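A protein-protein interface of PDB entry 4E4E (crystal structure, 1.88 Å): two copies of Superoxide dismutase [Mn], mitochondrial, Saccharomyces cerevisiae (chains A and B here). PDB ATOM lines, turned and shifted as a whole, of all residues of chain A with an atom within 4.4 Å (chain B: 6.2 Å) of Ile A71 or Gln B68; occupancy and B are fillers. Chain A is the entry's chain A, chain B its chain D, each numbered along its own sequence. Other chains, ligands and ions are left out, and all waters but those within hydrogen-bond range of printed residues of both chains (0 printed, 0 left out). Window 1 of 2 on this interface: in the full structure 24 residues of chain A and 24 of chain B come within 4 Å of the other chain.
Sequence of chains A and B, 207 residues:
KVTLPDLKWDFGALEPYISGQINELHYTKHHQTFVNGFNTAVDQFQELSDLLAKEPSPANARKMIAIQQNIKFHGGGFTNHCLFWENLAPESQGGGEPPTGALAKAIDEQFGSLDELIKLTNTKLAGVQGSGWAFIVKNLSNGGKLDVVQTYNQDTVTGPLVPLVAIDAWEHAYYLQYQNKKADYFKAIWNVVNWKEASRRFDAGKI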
ATOM      1  N   PHE A  38      12.258 -22.131  11.744  1.00  0.00           N
ATOM      2  CA  PHE A  38      12.378 -20.726  11.388  1.00  0.00           C
ATOM      3  C   PHE A  38      13.723 -20.431  10.722  1.00  0.00           C
ATOM      4  O   PHE A  38      13.787 -19.736   9.686  1.00  0.00           O
ATOM      5  CB  PHE A  38      12.219 -19.845  12.629  1.00  0.00           C
ATOM      6  CG  PHE A  38      12.226 -18.379  12.323  1.00  0.00           C
ATOM      7  CD1 PHE A  38      11.311 -17.852  11.434  1.00  0.00           C
ATOM      8  CD2 PHE A  38      13.140 -17.524  12.924  1.00  0.00           C
ATOM      9  CE1 PHE A  38      11.302 -16.487  11.134  1.00  0.00           C
ATOM     10  CE2 PHE A  38      13.139 -16.160  12.631  1.00  0.00           C
ATOM     11  CZ  PHE A  38      12.216 -15.642  11.740  1.00  0.00           C
ATOM     12  N   ALA A  41      13.540 -21.931   7.208  1.00  0.00           N
ATOM     13  CA  ALA A  41      12.673 -21.149   6.333  1.00  0.00           C
ATOM     14  C   ALA A  41      13.345 -19.844   5.882  1.00  0.00           C
ATOM     15  O   ALA A  41      13.245 -19.448   4.709  1.00  0.00           O
ATOM     16  CB  ALA A  41      11.354 -20.866   7.021  1.00  0.00           C
ATOM     17  N   PHE A  45      14.464 -18.833   2.139  1.00  0.00           N
ATOM     18  CA  PHE A  45      14.016 -17.607   1.499  1.00  0.00           C
ATOM     19  C   PHE A  45      15.190 -16.790   0.970  1.00  0.00           C
ATOM     20  O   PHE A  45      15.070 -16.161  -0.075  1.00  0.00           O
ATOM     21  CB  PHE A  45      13.105 -16.755   2.385  1.00  0.00           C
ATOM     22  CG  PHE A  45      12.225 -15.829   1.596  1.00  0.00           C
ATOM     23  CD1 PHE A  45      10.969 -16.233   1.170  1.00  0.00           C
ATOM     24  CD2 PHE A  45      12.675 -14.576   1.227  1.00  0.00           C
ATOM     25  CE1 PHE A  45      10.183 -15.377   0.395  1.00  0.00           C
ATOM     26  CE2 PHE A  45      11.896 -13.712   0.478  1.00  0.00           C
ATOM     27  CZ  PHE A  45      10.638 -14.112   0.067  1.00  0.00           C
ATOM     28  N   ILE A  67       7.217 -20.776   0.576  1.00  0.00           N
ATOM     29  CA  ILE A  67       8.056 -20.682   1.792  1.00  0.00           C
ATOM     30  C   ILE A  67       7.509 -19.721   2.888  1.00  0.00           C
ATOM     31  O   ILE A  67       7.765 -19.898   4.115  1.00  0.00           O
ATOM     32  CB  ILE A  67       9.513 -20.322   1.413  1.00  0.00           C
ATOM     33  CG1 ILE A  67      10.072 -21.395   0.473  1.00  0.00           C
ATOM     34  CG2 ILE A  67      10.413 -20.210   2.617  1.00  0.00           C
ATOM     35  CD1 ILE A  67       9.881 -22.816   0.964  1.00  0.00           C
ATOM     36  N   GLN A  68       6.766 -18.701   2.453  1.00  0.00           N
ATOM     37  CA  GLN A  68       6.280 -17.757   3.455  1.00  0.00           C
ATOM     38  C   GLN A  68       5.378 -18.383   4.526  1.00  0.00           C
ATOM     39  O   GLN A  68       5.402 -17.902   5.670  1.00  0.00           O
ATOM     40  CB  GLN A  68       5.694 -16.463   2.852  1.00  0.00           C
ATOM     41  CG  GLN A  68       4.548 -16.640   1.874  1.00  0.00           C
ATOM     42  CD  GLN A  68       3.228 -16.967   2.544  1.00  0.00           C
ATOM     43  OE1 GLN A  68       2.853 -16.338   3.531  1.00  0.00           O
ATOM     44  NE2 GLN A  68       2.505 -17.937   1.992  1.00  0.00           N
ATOM     45  N   GLN A  69       4.652 -19.441   4.198  1.00  0.00           N
ATOM     46  CA  GLN A  69       3.806 -20.110   5.177  1.00  0.00           C
ATOM     47  C   GLN A  69       4.639 -20.652   6.337  1.00  0.00           C
ATOM     48  O   GLN A  69       4.224 -20.593   7.508  1.00  0.00           O
ATOM     49  CB  GLN A  69       3.054 -21.242   4.489  1.00  0.00           C
ATOM     50  CG  GLN A  69       1.925 -21.853   5.297  1.00  0.00           C
ATOM     51  CD  GLN A  69       1.316 -23.037   4.564  1.00  0.00           C
ATOM     52  OE1 GLN A  69       0.658 -22.871   3.527  1.00  0.00           O
ATOM     53  NE2 GLN A  69       1.561 -24.241   5.076  1.00  0.00           N
ATOM     54  N   ASN A  70       5.818 -21.177   6.001  1.00  0.00           N
ATOM     55  CA  ASN A  70       6.739 -21.703   7.002  1.00  0.00           C
ATOM     56  C   ASN A  70       7.412 -20.601   7.795  1.00  0.00           C
ATOM     57  O   ASN A  70       7.624 -20.748   8.998  1.00  0.00           O
ATOM     58  CB  ASN A  70       7.807 -22.577   6.349  1.00  0.00           C
ATOM     59  CG  ASN A  70       7.232 -23.821   5.742  1.00  0.00           C
ATOM     60  OD1 ASN A  70       6.153 -24.271   6.136  1.00  0.00           O
ATOM     61  ND2 ASN A  70       7.936 -24.390   4.771  1.00  0.00           N
ATOM     62  N   ILE A  71       7.784 -19.512   7.123  1.00  0.00           N
ATOM     63  CA  ILE A  71       8.326 -18.377   7.884  1.00  0.00           C
ATOM     64  C   ILE A  71       7.302 -17.871   8.906  1.00  0.00           C
ATOM     65  O   ILE A  71       7.643 -17.511  10.039  1.00  0.00           O
ATOM     66  CB  ILE A  71       8.737 -17.184   6.973  1.00  0.00           C
ATOM     67  CG1 ILE A  71       9.948 -17.544   6.099  1.00  0.00           C
ATOM     68  CG2 ILE A  71       9.091 -15.982   7.827  1.00  0.00           C
ATOM     69  CD1 ILE A  71      10.232 -16.531   4.972  1.00  0.00           C
ATOM     70  N   MLY A  72       6.037 -17.851   8.509  1.00  0.00           N
ATOM     71  CA  MLY A  72       4.992 -17.339   9.390  1.00  0.00           C
ATOM     72  CB  MLY A  72       3.724 -17.064   8.580  1.00  0.00           C
ATOM     73  CG  MLY A  72       2.492 -16.741   9.412  1.00  0.00           C
ATOM     74  CD  MLY A  72       1.266 -16.752   8.508  1.00  0.00           C
ATOM     75  CE  MLY A  72      -0.037 -16.615   9.284  1.00  0.00           C
ATOM     76  NZ  MLY A  72      -0.639 -15.231   9.413  1.00  0.00           N
ATOM     77  CH1 MLY A  72      -1.920 -15.239   8.688  1.00  0.00           C
ATOM     78  CH2 MLY A  72       0.199 -14.219   8.751  1.00  0.00           C
ATOM     79  C   MLY A  72       4.710 -18.301  10.551  1.00  0.00           C
ATOM     80  O   MLY A  72       4.627 -17.887  11.710  1.00  0.00           O
ATOM     81  N   PHE A  73       4.591 -19.586  10.240  1.00  0.00           N
ATOM     82  CA  PHE A  73       4.284 -20.570  11.272  1.00  0.00           C
ATOM     83  C   PHE A  73       5.434 -20.780  12.254  1.00  0.00           C
ATOM     84  O   PHE A  73       5.246 -20.776  13.476  1.00  0.00           O
ATOM     85  CB  PHE A  73       3.886 -21.892  10.621  1.00  0.00           C
ATOM     86  CG  PHE A  73       3.622 -22.986  11.596  1.00  0.00           C
ATOM     87  CD1 PHE A  73       2.542 -22.908  12.474  1.00  0.00           C
ATOM     88  CD2 PHE A  73       4.455 -24.098  11.647  1.00  0.00           C
ATOM     89  CE1 PHE A  73       2.296 -23.923  13.387  1.00  0.00           C
ATOM     90  CE2 PHE A  73       4.214 -25.121  12.557  1.00  0.00           C
ATOM     91  CZ  PHE A  73       3.130 -25.037  13.423  1.00  0.00           C
ATOM     92  N   HIS A  74       6.634 -20.979  11.726  1.00  0.00           N
ATOM     93  CA  HIS A  74       7.786 -21.215  12.586  1.00  0.00           C
ATOM     94  C   HIS A  74       8.246 -19.933  13.268  1.00  0.00           C
ATOM     95  O   HIS A  74       8.670 -19.964  14.421  1.00  0.00           O
ATOM     96  CB  HIS A  74       8.920 -21.885  11.803  1.00  0.00           C
ATOM     97  CG  HIS A  74       8.642 -23.319  11.471  1.00  0.00           C
ATOM     98  ND1 HIS A  74       8.609 -24.307  12.436  1.00  0.00           N
ATOM     99  CD2 HIS A  74       8.388 -23.931  10.295  1.00  0.00           C
ATOM    100  CE1 HIS A  74       8.336 -25.462  11.863  1.00  0.00           C
ATOM    101  NE2 HIS A  74       8.199 -25.272  10.564  1.00  0.00           N
ATOM    102  N   GLY A  75       8.139 -18.805  12.566  1.00  0.00           N
ATOM    103  CA  GLY A  75       8.494 -17.522  13.153  1.00  0.00           C
ATOM    104  C   GLY A  75       7.569 -17.238  14.314  1.00  0.00           C
ATOM    105  O   GLY A  75       8.003 -16.854  15.411  1.00  0.00           O
ATOM    106  N   GLY A  76       6.283 -17.472  14.066  1.00  0.00           N
ATOM    107  CA  GLY A  76       5.258 -17.329  15.081  1.00  0.00           C
ATOM    108  C   GLY A  76       5.487 -18.239  16.273  1.00  0.00           C
ATOM    109  O   GLY A  76       5.383 -17.807  17.411  1.00  0.00           O
ATOM    110  N   PHE B  45      12.165  -7.755   3.114  1.00  0.00           N
ATOM    111  CA  PHE B  45      12.598  -9.052   3.641  1.00  0.00           C
ATOM    112  C   PHE B  45      14.102  -9.120   3.773  1.00  0.00           C
ATOM    113  O   PHE B  45      14.631  -9.565   4.783  1.00  0.00           O
ATOM    114  CB  PHE B  45      12.208 -10.240   2.752  1.00  0.00           C
ATOM    115  CG  PHE B  45      13.023 -11.480   3.054  1.00  0.00           C
ATOM    116  CD1 PHE B  45      12.688 -12.287   4.135  1.00  0.00           C
ATOM    117  CD2 PHE B  45      14.161 -11.801   2.308  1.00  0.00           C
ATOM    118  CE1 PHE B  45      13.443 -13.407   4.452  1.00  0.00           C
ATOM    119  CE2 PHE B  45      14.939 -12.916   2.632  1.00  0.00           C
ATOM    120  CZ  PHE B  45      14.573 -13.724   3.700  1.00  0.00           C
ATOM    121  N   MLY B  63       9.028  -8.755  13.437  1.00  0.00           N
ATOM    122  CA  MLY B  63       9.055  -7.835  12.297  1.00  0.00           C
ATOM    123  CB  MLY B  63      10.302  -6.952  12.342  1.00  0.00           C
ATOM    124  CG  MLY B  63      10.245  -5.850  13.390  1.00  0.00           C
ATOM    125  CD  MLY B  63      11.601  -5.155  13.479  1.00  0.00           C
ATOM    126  CE  MLY B  63      11.551  -4.003  14.473  1.00  0.00           C
ATOM    127  NZ  MLY B  63      12.659  -4.068  15.468  1.00  0.00           N
ATOM    128  CH1 MLY B  63      12.070  -3.826  16.800  1.00  0.00           C
ATOM    129  CH2 MLY B  63      13.547  -2.939  15.154  1.00  0.00           C
ATOM    130  C   MLY B  63       8.992  -8.575  10.957  1.00  0.00           C
ATOM    131  O   MLY B  63       8.275  -8.149  10.050  1.00  0.00           O
ATOM    132  N   MET B  64       9.727  -9.680  10.829  1.00  0.00           N
ATOM    133  CA  MET B  64       9.616 -10.495   9.599  1.00  0.00           C
ATOM    134  C   MET B  64       8.238 -11.127   9.373  1.00  0.00           C
ATOM    135  O   MET B  64       7.688 -11.176   8.221  1.00  0.00           O
ATOM    136  CB  MET B  64      10.670 -11.584   9.626  1.00  0.00           C
ATOM    137  CG  MET B  64      12.060 -11.020   9.754  1.00  0.00           C
ATOM    138  SD  MET B  64      13.231 -12.357   9.984  1.00  0.00           S
ATOM    139  CE  MET B  64      12.524 -13.545   8.843  1.00  0.00           C
ATOM    140  N   ILE B  65       7.693 -11.638  10.480  1.00  0.00           N
ATOM    141  CA  ILE B  65       6.353 -12.199  10.468  1.00  0.00           C
ATOM    142  C   ILE B  65       5.434 -11.161   9.855  1.00  0.00           C
ATOM    143  O   ILE B  65       4.651 -11.476   8.968  1.00  0.00           O
ATOM    144  CB  ILE B  65       5.861 -12.555  11.889  1.00  0.00           C
ATOM    145  CG1 ILE B  65       6.768 -13.623  12.512  1.00  0.00           C
ATOM    146  CG2 ILE B  65       4.423 -13.035  11.847  1.00  0.00           C
ATOM    147  CD1 ILE B  65       6.422 -13.945  13.969  1.00  0.00           C
ATOM    148  N   ALA B  66       5.560  -9.912  10.301  1.00  0.00           N
ATOM    149  CA  ALA B  66       4.749  -8.835   9.726  1.00  0.00           C
ATOM    150  C   ALA B  66       4.786  -8.685   8.178  1.00  0.00           C
ATOM    151  O   ALA B  66       3.762  -8.370   7.575  1.00  0.00           O
ATOM    152  CB  ALA B  66       5.080  -7.505  10.413  1.00  0.00           C
ATOM    153  N   ILE B  67       5.953  -8.910   7.555  1.00  0.00           N
ATOM    154  CA  ILE B  67       6.165  -8.705   6.105  1.00  0.00           C
ATOM    155  C   ILE B  67       5.710  -9.898   5.262  1.00  0.00           C
ATOM    156  O   ILE B  67       5.350  -9.772   4.059  1.00  0.00           O
ATOM    157  CB  ILE B  67       7.672  -8.467   5.812  1.00  0.00           C
ATOM    158  CG1 ILE B  67       8.155  -7.221   6.545  1.00  0.00           C
ATOM    159  CG2 ILE B  67       7.949  -8.304   4.331  1.00  0.00           C
ATOM    160  CD1 ILE B  67       7.387  -5.975   6.168  1.00  0.00           C
ATOM    161  N   GLN B  68       5.728 -11.073   5.885  1.00  0.00           N
ATOM    162  CA  GLN B  68       5.284 -12.295   5.198  1.00  0.00           C
ATOM    163  C   GLN B  68       3.954 -12.135   4.471  1.00  0.00           C
ATOM    164  O   GLN B  68       3.762 -12.639   3.351  1.00  0.00           O
ATOM    165  CB  GLN B  68       5.182 -13.459   6.187  1.00  0.00           C
ATOM    166  CG  GLN B  68       6.503 -13.788   6.812  1.00  0.00           C
ATOM    167  CD  GLN B  68       7.633 -13.661   5.820  1.00  0.00           C
ATOM    168  OE1 GLN B  68       7.726 -14.436   4.870  1.00  0.00           O
ATOM    169  NE2 GLN B  68       8.497 -12.672   6.026  1.00  0.00           N
ATOM    170  N   GLN B  69       3.009 -11.450   5.119  1.00  0.00           N
ATOM    171  CA  GLN B  69       1.687 -11.245   4.520  1.00  0.00           C
ATOM    172  C   GLN B  69       1.733 -10.475   3.183  1.00  0.00           C
ATOM    173  O   GLN B  69       1.040 -10.831   2.217  1.00  0.00           O
ATOM    174  CB  GLN B  69       0.746 -10.535   5.503  1.00  0.00           C
ATOM    175  CG  GLN B  69      -0.452  -9.852   4.832  1.00  0.00           C
ATOM    176  CD  GLN B  69      -1.672  -9.746   5.737  1.00  0.00           C
ATOM    177  OE1 GLN B  69      -1.955 -10.652   6.531  1.00  0.00           O
ATOM    178  NE2 GLN B  69      -2.406  -8.642   5.615  1.00  0.00           N
ATOM    179  N   ASN B  70       2.536  -9.418   3.127  1.00  0.00           N
ATOM    180  CA  ASN B  70       2.697  -8.675   1.877  1.00  0.00           C
ATOM    181  C   ASN B  70       3.421  -9.495   0.827  1.00  0.00           C
ATOM    182  O   ASN B  70       3.104  -9.401  -0.367  1.00  0.00           O
ATOM    183  CB  ASN B  70       3.437  -7.358   2.106  1.00  0.00           C
ATOM    184  CG  ASN B  70       2.613  -6.360   2.887  1.00  0.00           C
ATOM    185  OD1 ASN B  70       1.379  -6.439   2.921  1.00  0.00           O
ATOM    186  ND2 ASN B  70       3.289  -5.415   3.529  1.00  0.00           N
ATOM    187  N   ILE B  71       4.400 -10.288   1.250  1.00  0.00           N
ATOM    188  CA  ILE B  71       5.059 -11.142   0.253  1.00  0.00           C
ATOM    189  C   ILE B  71       4.033 -12.099  -0.348  1.00  0.00           C
ATOM    190  O   ILE B  71       4.006 -12.305  -1.556  1.00  0.00           O
ATOM    191  CB  ILE B  71       6.261 -11.948   0.821  1.00  0.00           C
ATOM    192  CG1 ILE B  71       7.408 -11.014   1.212  1.00  0.00           C
ATOM    193  CG2 ILE B  71       6.778 -12.939  -0.210  1.00  0.00           C
ATOM    194  CD1 ILE B  71       8.552 -11.734   1.899  1.00  0.00           C
ATOM    195  N   MLY B  72       3.154 -12.646   0.489  1.00  0.00           N
ATOM    196  CA  MLY B  72       2.156 -13.588  -0.011  1.00  0.00           C
ATOM    197  CB  MLY B  72       1.485 -14.296   1.167  1.00  0.00           C
ATOM    198  CG  MLY B  72       0.593 -15.456   0.769  1.00  0.00           C
ATOM    199  CD  MLY B  72      -0.348 -15.788   1.916  1.00  0.00           C
ATOM    200  CE  MLY B  72      -0.978 -17.161   1.722  1.00  0.00           C
ATOM    201  NZ  MLY B  72      -1.953 -17.461   2.816  1.00  0.00           N
ATOM    202  CH1 MLY B  72      -2.734 -18.620   2.355  1.00  0.00           C
ATOM    203  CH2 MLY B  72      -2.877 -16.314   2.900  1.00  0.00           C
ATOM    204  C   MLY B  72       1.108 -12.938  -0.917  1.00  0.00           C
ATOM    205  O   MLY B  72       0.762 -13.476  -1.968  1.00  0.00           O
ATOM    206  N   PHE B  73       0.606 -11.777  -0.509  1.00  0.00           N
ATOM    207  CA  PHE B  73      -0.430 -11.089  -1.273  1.00  0.00           C
ATOM    208  C   PHE B  73       0.092 -10.562  -2.594  1.00  0.00           C
ATOM    209  O   PHE B  73      -0.533 -10.744  -3.644  1.00  0.00           O
ATOM    210  CB  PHE B  73      -1.013  -9.941  -0.452  1.00  0.00           C
ATOM    211  CG  PHE B  73      -2.077  -9.162  -1.168  1.00  0.00           C
ATOM    212  CD1 PHE B  73      -3.306  -9.750  -1.479  1.00  0.00           C
ATOM    213  CD2 PHE B  73      -1.863  -7.833  -1.509  1.00  0.00           C
ATOM    214  CE1 PHE B  73      -4.305  -9.021  -2.128  1.00  0.00           C
ATOM    215  CE2 PHE B  73      -2.859  -7.090  -2.158  1.00  0.00           C
ATOM    216  CZ  PHE B  73      -4.080  -7.688  -2.469  1.00  0.00           C
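O of Met B64 is in hydrogen-bond range of NE2 of Gln B68 (2.8 Å).
Of the printed residues of chain A, Gln B68 touches Gln A68 and Ile A71.
Printed residues of chain B within 4 Å of Phe A45: Phe B45 (3.1 Å) and Ile B71 (3.7 Å).
Printed residues of chain A within 4 Å of Phe B45: Phe A45 (3.1 Å).
The nearest printed residue of chain B that does not touch Ile A71 is Met B64 (4.3 Å).
The nearest printed residue of chain A that does not touch Gln B68 is MLY A72 (4.4 Å).
The nearest printed residue of chain A that does not touch Ile B65 is Ile A71 (4.7 Å).
Phe A38 touches Met B64 (CZ to CE, 3.6 Å).
Phe B45 touches Phe A45 (CE2 to CD2, 3.1 Å).
CZ of Phe A45 touches CD1 of Ile B71, at 3.7 Å.
Gln A68 touches Gln B68.
CG of MLY B72 touches NE2 of Gln A68 (3.4 Å).
CD1 of Ile A71 touches OE1 of Gln B68, at 3.3 Å.
CD1 of Ile B65 touches C of Gly A75, 3.5 Å away.
Ile B65 touches Gly A76.
Phe A45 touches its own counterpart, Phe B45.
Phe A45 touches Ile B71, but with the chains exchanged Ile A71 does not touch Phe B45 (4.5 Å).
Gln B68 touches its own counterpart, Gln A68.
Ile A71 touches Gln B68, but with the chains exchanged Gln A68 does not touch Ile B71 (4.8 Å).
Positions printed for both chains: 45, 67, 68, 69, 70, 71, 72 and 73.
Of the 8 pairs that touch across the chains among the printed residues, 2 have their exchanged pair printed and touching as well.
Of the 13 printed residues of chain A, 6 touch a printed residue of chain B.
Printed residues of chain A that touch a printed residue of chain B: Phe A38, Phe A45, Gln A68, Ile A71, Gly A75 and Gly A76.
Among the printed residues, no Asp or Glu carboxylate lies within 4 Å of a Lys or Arg side-chain nitrogen of the other chain.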
